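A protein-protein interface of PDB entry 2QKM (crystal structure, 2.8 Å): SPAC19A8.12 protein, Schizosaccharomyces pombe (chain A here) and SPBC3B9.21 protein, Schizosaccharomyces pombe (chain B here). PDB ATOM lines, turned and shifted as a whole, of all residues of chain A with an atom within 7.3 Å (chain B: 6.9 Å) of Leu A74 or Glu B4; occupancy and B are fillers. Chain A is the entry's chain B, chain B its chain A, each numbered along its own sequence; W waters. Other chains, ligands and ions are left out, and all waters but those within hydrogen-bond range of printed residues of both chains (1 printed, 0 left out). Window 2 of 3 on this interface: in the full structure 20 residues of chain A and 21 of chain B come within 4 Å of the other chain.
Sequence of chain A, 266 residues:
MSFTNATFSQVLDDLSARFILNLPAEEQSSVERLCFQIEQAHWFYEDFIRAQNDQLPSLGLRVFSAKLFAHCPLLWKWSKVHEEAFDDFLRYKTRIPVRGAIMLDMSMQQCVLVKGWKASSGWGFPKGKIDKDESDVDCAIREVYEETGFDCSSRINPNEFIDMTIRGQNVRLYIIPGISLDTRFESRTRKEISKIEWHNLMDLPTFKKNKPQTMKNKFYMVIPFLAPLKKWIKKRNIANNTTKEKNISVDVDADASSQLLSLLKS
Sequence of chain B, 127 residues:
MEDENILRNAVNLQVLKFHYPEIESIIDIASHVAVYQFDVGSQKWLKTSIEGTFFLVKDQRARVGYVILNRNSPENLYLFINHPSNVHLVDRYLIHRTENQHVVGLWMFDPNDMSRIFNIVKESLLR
Of the 16 printed residues of chain A, 5 touch a printed residue of chain B.
Along chain B the printed residues that touch a printed residue of chain A span positions 1 to 8.
Of the printed residues of chain B, Leu A74 touches Glu B4 and Arg B8.
Glu B4 touches just these residues of chain A: Pro A73 (3.9 Å), Leu A74 (3.9 Å) and Lys A77 (3.1 Å).
Of the printed residues of chain A, Leu B7 touches Pro A73.
Printed residues of chain A within 4 Å of Arg B8: Leu A21, Asn A22 and Leu A74.
The nearest printed residue of chain B that does not touch Leu A74 is Asn B5 (4.002 Å).
The nearest residue of chain A that does not touch Glu B4 is Leu A75 (5.8 Å).
The nearest printed residue of chain A that does not touch Leu B7 is Trp A76 (4.1 Å).
Among the printed residues, pairs that only touch across the chains: Leu A74 with Arg B8, Asn A22 with Arg B8, Pro A73 with Leu B7, Pro A73 with Glu B4 and Leu A74 with Glu B4.
The side-chain sulfur (SD) of Met B1 lies close to the backbone NH (N) of Asp B3, at 3.6 Å.
The backbone carbonyl oxygen (O) of Leu A21 lies close to the side-chain amide oxygen (OE1) of Gln A28, at 3.2 Å.
The side-chain amino group of Lys A77 lies within salt-bridge range of the side-chain carboxylate of Glu B4 (3.1 Å).
NE of Arg B8 sits close to O of Leu A21 (3.4 Å).
N of Met B1 sits close to NZ of Lys A77, 2.9 Å away.
Water W1 lies within hydrogen-bond range of NH1 of Arg B8 and ND2 of Asn A22.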
ATOM      1  N   ILE A  20      -4.016   6.395  31.972  1.00  0.00           N
ATOM      2  CA  ILE A  20      -3.950   5.504  30.808  1.00  0.00           C
ATOM      3  C   ILE A  20      -5.266   4.848  30.377  1.00  0.00           C
ATOM      4  O   ILE A  20      -5.537   4.731  29.181  1.00  0.00           O
ATOM      5  CB  ILE A  20      -2.871   4.402  30.979  1.00  0.00           C
ATOM      6  CG1 ILE A  20      -3.206   3.472  32.159  1.00  0.00           C
ATOM      7  CG2 ILE A  20      -1.506   5.027  31.121  1.00  0.00           C
ATOM      8  CD1 ILE A  20      -2.526   2.090  32.088  1.00  0.00           C
ATOM      9  N   LEU A  21      -6.071   4.409  31.338  1.00  0.00           N
ATOM     10  CA  LEU A  21      -7.331   3.711  31.049  1.00  0.00           C
ATOM     11  C   LEU A  21      -8.252   4.340  29.978  1.00  0.00           C
ATOM     12  O   LEU A  21      -8.828   3.637  29.162  1.00  0.00           O
ATOM     13  CB  LEU A  21      -8.119   3.487  32.345  1.00  0.00           C
ATOM     14  CG  LEU A  21      -9.391   2.635  32.272  1.00  0.00           C
ATOM     15  CD1 LEU A  21      -9.148   1.330  31.532  1.00  0.00           C
ATOM     16  CD2 LEU A  21      -9.923   2.349  33.670  1.00  0.00           C
ATOM     17  N   ASN A  22      -8.404   5.655  29.995  1.00  0.00           N
ATOM     18  CA  ASN A  22      -9.366   6.318  29.130  1.00  0.00           C
ATOM     19  C   ASN A  22      -8.747   7.061  27.949  1.00  0.00           C
ATOM     20  O   ASN A  22      -9.369   7.952  27.353  1.00  0.00           O
ATOM     21  CB  ASN A  22     -10.210   7.252  29.973  1.00  0.00           C
ATOM     22  CG  ASN A  22     -10.916   6.525  31.067  1.00  0.00           C
ATOM     23  OD1 ASN A  22     -10.634   6.735  32.244  1.00  0.00           O
ATOM     24  ND2 ASN A  22     -11.832   5.642  30.692  1.00  0.00           N
ATOM     25  N   LEU A  23      -7.522   6.680  27.610  1.00  0.00           N
ATOM     26  CA  LEU A  23      -6.855   7.216  26.453  1.00  0.00           C
ATOM     27  C   LEU A  23      -7.537   6.706  25.210  1.00  0.00           C
ATOM     28  O   LEU A  23      -8.176   5.665  25.254  1.00  0.00           O
ATOM     29  CB  LEU A  23      -5.400   6.782  26.437  1.00  0.00           C
ATOM     30  CG  LEU A  23      -4.480   7.450  27.455  1.00  0.00           C
ATOM     31  CD1 LEU A  23      -3.213   6.630  27.556  1.00  0.00           C
ATOM     32  CD2 LEU A  23      -4.189   8.873  27.063  1.00  0.00           C
ATOM     33  N   ALA A  25      -7.728   4.555  22.044  1.00  0.00           N
ATOM     34  CA  ALA A  25      -7.081   3.290  21.721  1.00  0.00           C
ATOM     35  C   ALA A  25      -5.729   3.466  21.027  1.00  0.00           C
ATOM     36  O   ALA A  25      -4.760   2.806  21.401  1.00  0.00           O
ATOM     37  CB  ALA A  25      -7.981   2.441  20.885  1.00  0.00           C
ATOM     38  N   GLN A  28      -2.949   4.220  23.405  1.00  0.00           N
ATOM     39  CA  GLN A  28      -2.580   3.033  24.171  1.00  0.00           C
ATOM     40  C   GLN A  28      -1.656   2.124  23.337  1.00  0.00           C
ATOM     41  O   GLN A  28      -0.786   1.428  23.873  1.00  0.00           O
ATOM     42  CB  GLN A  28      -3.835   2.294  24.647  1.00  0.00           C
ATOM     43  CG  GLN A  28      -4.623   3.068  25.690  1.00  0.00           C
ATOM     44  CD  GLN A  28      -5.966   2.467  26.072  1.00  0.00           C
ATOM     45  OE1 GLN A  28      -6.471   2.743  27.156  1.00  0.00           O
ATOM     46  NE2 GLN A  28      -6.553   1.658  25.195  1.00  0.00           N
ATOM     47  N   SER A  29      -1.815   2.170  22.021  1.00  0.00           N
ATOM     48  CA  SER A  29      -1.001   1.360  21.142  1.00  0.00           C
ATOM     49  C   SER A  29       0.297   2.030  20.732  1.00  0.00           C
ATOM     50  O   SER A  29       1.121   1.431  20.041  1.00  0.00           O
ATOM     51  CB  SER A  29      -1.804   0.922  19.924  1.00  0.00           C
ATOM     52  OG  SER A  29      -2.319  -0.384  20.146  1.00  0.00           O
ATOM     53  N   PHE A  69      -0.455  -2.013  34.545  1.00  0.00           N
ATOM     54  CA  PHE A  69      -1.087  -2.813  33.491  1.00  0.00           C
ATOM     55  C   PHE A  69      -2.161  -3.762  34.038  1.00  0.00           C
ATOM     56  O   PHE A  69      -3.207  -3.973  33.409  1.00  0.00           O
ATOM     57  CB  PHE A  69      -0.050  -3.585  32.659  1.00  0.00           C
ATOM     58  CG  PHE A  69       0.554  -2.779  31.530  1.00  0.00           C
ATOM     59  CD1 PHE A  69       0.991  -1.478  31.729  1.00  0.00           C
ATOM     60  CD2 PHE A  69       0.733  -3.344  30.286  1.00  0.00           C
ATOM     61  CE1 PHE A  69       1.570  -0.751  30.692  1.00  0.00           C
ATOM     62  CE2 PHE A  69       1.307  -2.612  29.241  1.00  0.00           C
ATOM     63  CZ  PHE A  69       1.721  -1.317  29.440  1.00  0.00           C
ATOM     64  N   HIS A  71      -4.198  -3.136  36.159  1.00  0.00           N
ATOM     65  CA  HIS A  71      -5.448  -2.417  36.374  1.00  0.00           C
ATOM     66  C   HIS A  71      -5.922  -1.677  35.121  1.00  0.00           C
ATOM     67  O   HIS A  71      -6.686  -0.699  35.206  1.00  0.00           O
ATOM     68  CB  HIS A  71      -5.355  -1.501  37.589  1.00  0.00           C
ATOM     69  CG  HIS A  71      -5.062  -2.230  38.864  1.00  0.00           C
ATOM     70  ND1 HIS A  71      -5.970  -2.322  39.897  1.00  0.00           N
ATOM     71  CD2 HIS A  71      -3.959  -2.905  39.273  1.00  0.00           C
ATOM     72  CE1 HIS A  71      -5.440  -3.019  40.887  1.00  0.00           C
ATOM     73  NE2 HIS A  71      -4.218  -3.384  40.534  1.00  0.00           N
ATOM     74  N   CYS A  72      -5.500  -2.179  33.959  1.00  0.00           N
ATOM     75  CA  CYS A  72      -5.855  -1.575  32.678  1.00  0.00           C
ATOM     76  C   CYS A  72      -6.289  -2.586  31.609  1.00  0.00           C
ATOM     77  O   CYS A  72      -5.469  -3.024  30.807  1.00  0.00           O
ATOM     78  CB  CYS A  72      -4.685  -0.746  32.166  1.00  0.00           C
ATOM     79  SG  CYS A  72      -5.168   0.264  30.777  1.00  0.00           S
ATOM     80  N   PRO A  73      -7.587  -2.935  31.571  1.00  0.00           N
ATOM     81  CA  PRO A  73      -8.144  -4.002  30.734  1.00  0.00           C
ATOM     82  C   PRO A  73      -7.787  -3.920  29.249  1.00  0.00           C
ATOM     83  O   PRO A  73      -7.572  -4.947  28.607  1.00  0.00           O
ATOM     84  CB  PRO A  73      -9.649  -3.820  30.895  1.00  0.00           C
ATOM     85  CG  PRO A  73      -9.817  -3.153  32.187  1.00  0.00           C
ATOM     86  CD  PRO A  73      -8.630  -2.274  32.370  1.00  0.00           C
ATOM     87  N   LEU A  74      -7.721  -2.713  28.712  1.00  0.00           N
ATOM     88  CA  LEU A  74      -7.451  -2.511  27.296  1.00  0.00           C
ATOM     89  C   LEU A  74      -6.033  -2.883  26.894  1.00  0.00           C
ATOM     90  O   LEU A  74      -5.709  -2.947  25.702  1.00  0.00           O
ATOM     91  CB  LEU A  74      -7.700  -1.054  26.948  1.00  0.00           C
ATOM     92  CG  LEU A  74      -9.059  -0.562  27.439  1.00  0.00           C
ATOM     93  CD1 LEU A  74      -8.867   0.855  27.850  1.00  0.00           C
ATOM     94  CD2 LEU A  74     -10.112  -0.692  26.358  1.00  0.00           C
ATOM     95  N   LEU A  75      -5.186  -3.119  27.887  1.00  0.00           N
ATOM     96  CA  LEU A  75      -3.823  -3.525  27.615  1.00  0.00           C
ATOM     97  C   LEU A  75      -3.649  -5.055  27.697  1.00  0.00           C
ATOM     98  O   LEU A  75      -2.582  -5.581  27.373  1.00  0.00           O
ATOM     99  CB  LEU A  75      -2.846  -2.763  28.519  1.00  0.00           C
ATOM    100  CG  LEU A  75      -2.858  -1.220  28.442  1.00  0.00           C
ATOM    101  CD1 LEU A  75      -1.785  -0.608  29.339  1.00  0.00           C
ATOM    102  CD2 LEU A  75      -2.712  -0.675  27.026  1.00  0.00           C
ATOM    103  N   TRP A  76      -4.713  -5.767  28.080  1.00  0.00           N
ATOM    104  CA  TRP A  76      -4.647  -7.222  28.275  1.00  0.00           C
ATOM    105  C   TRP A  76      -4.762  -8.021  26.977  1.00  0.00           C
ATOM    106  O   TRP A  76      -4.724  -9.248  26.982  1.00  0.00           O
ATOM    107  CB  TRP A  76      -5.732  -7.695  29.249  1.00  0.00           C
ATOM    108  CG  TRP A  76      -5.706  -7.055  30.596  1.00  0.00           C
ATOM    109  CD1 TRP A  76      -4.739  -6.252  31.105  1.00  0.00           C
ATOM    110  CD2 TRP A  76      -6.692  -7.191  31.622  1.00  0.00           C
ATOM    111  NE1 TRP A  76      -5.065  -5.857  32.379  1.00  0.00           N
ATOM    112  CE2 TRP A  76      -6.259  -6.424  32.723  1.00  0.00           C
ATOM    113  CE3 TRP A  76      -7.904  -7.884  31.717  1.00  0.00           C
ATOM    114  CZ2 TRP A  76      -6.990  -6.326  33.904  1.00  0.00           C
ATOM    115  CZ3 TRP A  76      -8.637  -7.783  32.898  1.00  0.00           C
ATOM    116  CH2 TRP A  76      -8.174  -7.010  33.975  1.00  0.00           C
ATOM    117  N   LYS A  77      -4.915  -7.333  25.860  1.00  0.00           N
ATOM    118  CA  LYS A  77      -5.196  -8.022  24.620  1.00  0.00           C
ATOM    119  C   LYS A  77      -3.910  -8.159  23.834  1.00  0.00           C
ATOM    120  O   LYS A  77      -3.916  -8.468  22.643  1.00  0.00           O
ATOM    121  CB  LYS A  77      -6.220  -7.220  23.822  1.00  0.00           C
ATOM    122  CG  LYS A  77      -7.200  -8.045  23.022  1.00  0.00           C
ATOM    123  CD  LYS A  77      -8.029  -7.158  22.107  1.00  0.00           C
ATOM    124  CE  LYS A  77      -9.287  -6.629  22.774  1.00  0.00           C
ATOM    125  NZ  LYS A  77     -10.175  -5.914  21.786  1.00  0.00           N
ATOM    126  N   TRP A  78      -2.783  -7.942  24.492  1.00  0.00           N
ATOM    127  CA  TRP A  78      -1.576  -7.805  23.703  1.00  0.00           C
ATOM    128  C   TRP A  78      -0.389  -8.748  23.984  1.00  0.00           C
ATOM    129  O   TRP A  78      -0.244  -9.282  25.093  1.00  0.00           O
ATOM    130  CB  TRP A  78      -1.255  -6.313  23.466  1.00  0.00           C
ATOM    131  CG  TRP A  78      -0.305  -5.572  24.349  1.00  0.00           C
ATOM    132  CD1 TRP A  78       0.726  -6.080  25.072  1.00  0.00           C
ATOM    133  CD2 TRP A  78      -0.230  -4.137  24.489  1.00  0.00           C
ATOM    134  NE1 TRP A  78       1.425  -5.055  25.685  1.00  0.00           N
ATOM    135  CE2 TRP A  78       0.861  -3.855  25.340  1.00  0.00           C
ATOM    136  CE3 TRP A  78      -0.981  -3.074  23.978  1.00  0.00           C
ATOM    137  CZ2 TRP A  78       1.213  -2.551  25.708  1.00  0.00           C
ATOM    138  CZ3 TRP A  78      -0.638  -1.790  24.336  1.00  0.00           C
ATOM    139  CH2 TRP A  78       0.451  -1.534  25.202  1.00  0.00           C
ATOM    140  N   MET B   1     -12.674  -7.310  21.446  1.00  0.00           N
ATOM    141  CA  MET B   1     -13.782  -7.860  22.283  1.00  0.00           C
ATOM    142  C   MET B   1     -14.370  -6.777  23.186  1.00  0.00           C
ATOM    143  O   MET B   1     -13.662  -5.868  23.616  1.00  0.00           O
ATOM    144  CB  MET B   1     -13.283  -9.043  23.124  1.00  0.00           C
ATOM    145  CG  MET B   1     -14.217 -10.250  23.131  1.00  0.00           C
ATOM    146  SD  MET B   1     -15.881  -9.912  23.761  1.00  0.00           S
ATOM    147  CE  MET B   1     -16.614 -11.549  23.598  1.00  0.00           C
ATOM    148  N   GLU B   2     -15.667  -6.893  23.466  1.00  0.00           N
ATOM    149  CA  GLU B   2     -16.400  -5.908  24.270  1.00  0.00           C
ATOM    150  C   GLU B   2     -16.150  -6.042  25.775  1.00  0.00           C
ATOM    151  O   GLU B   2     -16.366  -5.087  26.521  1.00  0.00           O
ATOM    152  CB  GLU B   2     -17.908  -5.973  23.974  1.00  0.00           C
ATOM    153  CG  GLU B   2     -18.546  -7.363  24.173  1.00  0.00           C
ATOM    154  CD  GLU B   2     -19.994  -7.308  24.678  1.00  0.00           C
ATOM    155  OE1 GLU B   2     -20.578  -8.390  24.913  1.00  0.00           O
ATOM    156  OE2 GLU B   2     -20.549  -6.196  24.841  1.00  0.00           O
ATOM    157  N   ASP B   3     -15.707  -7.225  26.209  1.00  0.00           N
ATOM    158  CA  ASP B   3     -15.373  -7.486  27.615  1.00  0.00           C
ATOM    159  C   ASP B   3     -14.553  -6.363  28.234  1.00  0.00           C
ATOM    160  O   ASP B   3     -14.880  -5.883  29.320  1.00  0.00           O
ATOM    161  CB  ASP B   3     -14.624  -8.811  27.770  1.00  0.00           C
ATOM    162  CG  ASP B   3     -15.545  -9.976  28.093  1.00  0.00           C
ATOM    163  OD1 ASP B   3     -16.488  -9.787  28.899  1.00  0.00           O
ATOM    164  OD2 ASP B   3     -15.313 -11.086  27.555  1.00  0.00           O
ATOM    165  N   GLU B   4     -13.505  -5.944  27.527  1.00  0.00           N
ATOM    166  CA  GLU B   4     -12.640  -4.847  27.966  1.00  0.00           C
ATOM    167  C   GLU B   4     -13.402  -3.565  28.336  1.00  0.00           C
ATOM    168  O   GLU B   4     -13.061  -2.899  29.305  1.00  0.00           O
ATOM    169  CB  GLU B   4     -11.564  -4.551  26.914  1.00  0.00           C
ATOM    170  CG  GLU B   4     -12.111  -4.104  25.567  1.00  0.00           C
ATOM    171  CD  GLU B   4     -11.048  -4.008  24.483  1.00  0.00           C
ATOM    172  OE1 GLU B   4      -9.868  -4.358  24.744  1.00  0.00           O
ATOM    173  OE2 GLU B   4     -11.397  -3.571  23.359  1.00  0.00           O
ATOM    174  N   ASN B   5     -14.435  -3.236  27.571  1.00  0.00           N
ATOM    175  CA  ASN B   5     -15.250  -2.069  27.872  1.00  0.00           C
ATOM    176  C   ASN B   5     -16.095  -2.252  29.122  1.00  0.00           C
ATOM    177  O   ASN B   5     -16.097  -1.384  29.980  1.00  0.00           O
ATOM    178  CB  ASN B   5     -16.101  -1.646  26.674  1.00  0.00           C
ATOM    179  CG  ASN B   5     -15.268  -1.091  25.538  1.00  0.00           C
ATOM    180  OD1 ASN B   5     -15.781  -0.436  24.652  1.00  0.00           O
ATOM    181  ND2 ASN B   5     -13.978  -1.354  25.563  1.00  0.00           N
ATOM    182  N   ILE B   6     -16.796  -3.379  29.242  1.00  0.00           N
ATOM    183  CA  ILE B   6     -17.528  -3.670  30.485  1.00  0.00           C
ATOM    184  C   ILE B   6     -16.579  -3.534  31.679  1.00  0.00           C
ATOM    185  O   ILE B   6     -16.928  -2.909  32.692  1.00  0.00           O
ATOM    186  CB  ILE B   6     -18.243  -5.062  30.471  1.00  0.00           C
ATOM    187  CG1 ILE B   6     -19.519  -5.009  29.620  1.00  0.00           C
ATOM    188  CG2 ILE B   6     -18.646  -5.500  31.877  1.00  0.00           C
ATOM    189  CD1 ILE B   6     -19.323  -5.385  28.156  1.00  0.00           C
ATOM    190  N   LEU B   7     -15.380  -4.101  31.535  1.00  0.00           N
ATOM    191  CA  LEU B   7     -14.303  -3.946  32.520  1.00  0.00           C
ATOM    192  C   LEU B   7     -13.860  -2.490  32.733  1.00  0.00           C
ATOM    193  O   LEU B   7     -13.772  -2.046  33.873  1.00  0.00           O
ATOM    194  CB  LEU B   7     -13.105  -4.835  32.157  1.00  0.00           C
ATOM    195  CG  LEU B   7     -12.927  -6.246  32.742  1.00  0.00           C
ATOM    196  CD1 LEU B   7     -14.151  -6.773  33.487  1.00  0.00           C
ATOM    197  CD2 LEU B   7     -12.477  -7.229  31.658  1.00  0.00           C
ATOM    198  N   ARG B   8     -13.616  -1.751  31.645  1.00  0.00           N
ATOM    199  CA  ARG B   8     -13.215  -0.333  31.719  1.00  0.00           C
ATOM    200  C   ARG B   8     -14.257   0.569  32.397  1.00  0.00           C
ATOM    201  O   ARG B   8     -13.896   1.544  33.062  1.00  0.00           O
ATOM    202  CB  ARG B   8     -12.825   0.218  30.334  1.00  0.00           C
ATOM    203  CG  ARG B   8     -13.069   1.719  30.143  1.00  0.00           C
ATOM    204  CD  ARG B   8     -11.906   2.492  29.488  1.00  0.00           C
ATOM    205  NE  ARG B   8     -11.638   2.092  28.100  1.00  0.00           N
ATOM    206  CZ  ARG B   8     -12.338   2.500  27.052  1.00  0.00           C
ATOM    207  NH1 ARG B   8     -13.347   3.330  27.223  1.00  0.00           N
ATOM    208  NH2 ARG B   8     -12.040   2.072  25.840  1.00  0.00           N
ATOM    209  N   ASN B   9     -15.534   0.239  32.219  1.00  0.00           N
ATOM    210  CA  ASN B   9     -16.613   0.989  32.831  1.00  0.00           C
ATOM    211  C   ASN B   9     -16.627   0.804  34.346  1.00  0.00           C
ATOM    212  O   ASN B   9     -16.651   1.776  35.095  1.00  0.00           O
ATOM    213  CB  ASN B   9     -17.962   0.590  32.223  1.00  0.00           C
ATOM    214  CG  ASN B   9     -18.003   0.769  30.703  1.00  0.00           C
ATOM    215  OD1 ASN B   9     -17.140   1.428  30.116  1.00  0.00           O
ATOM    216  ND2 ASN B   9     -19.003   0.173  30.060  1.00  0.00           N
HETATM  217  O   HOH W   1     -13.244   5.854  28.090  1.00  0.00           O
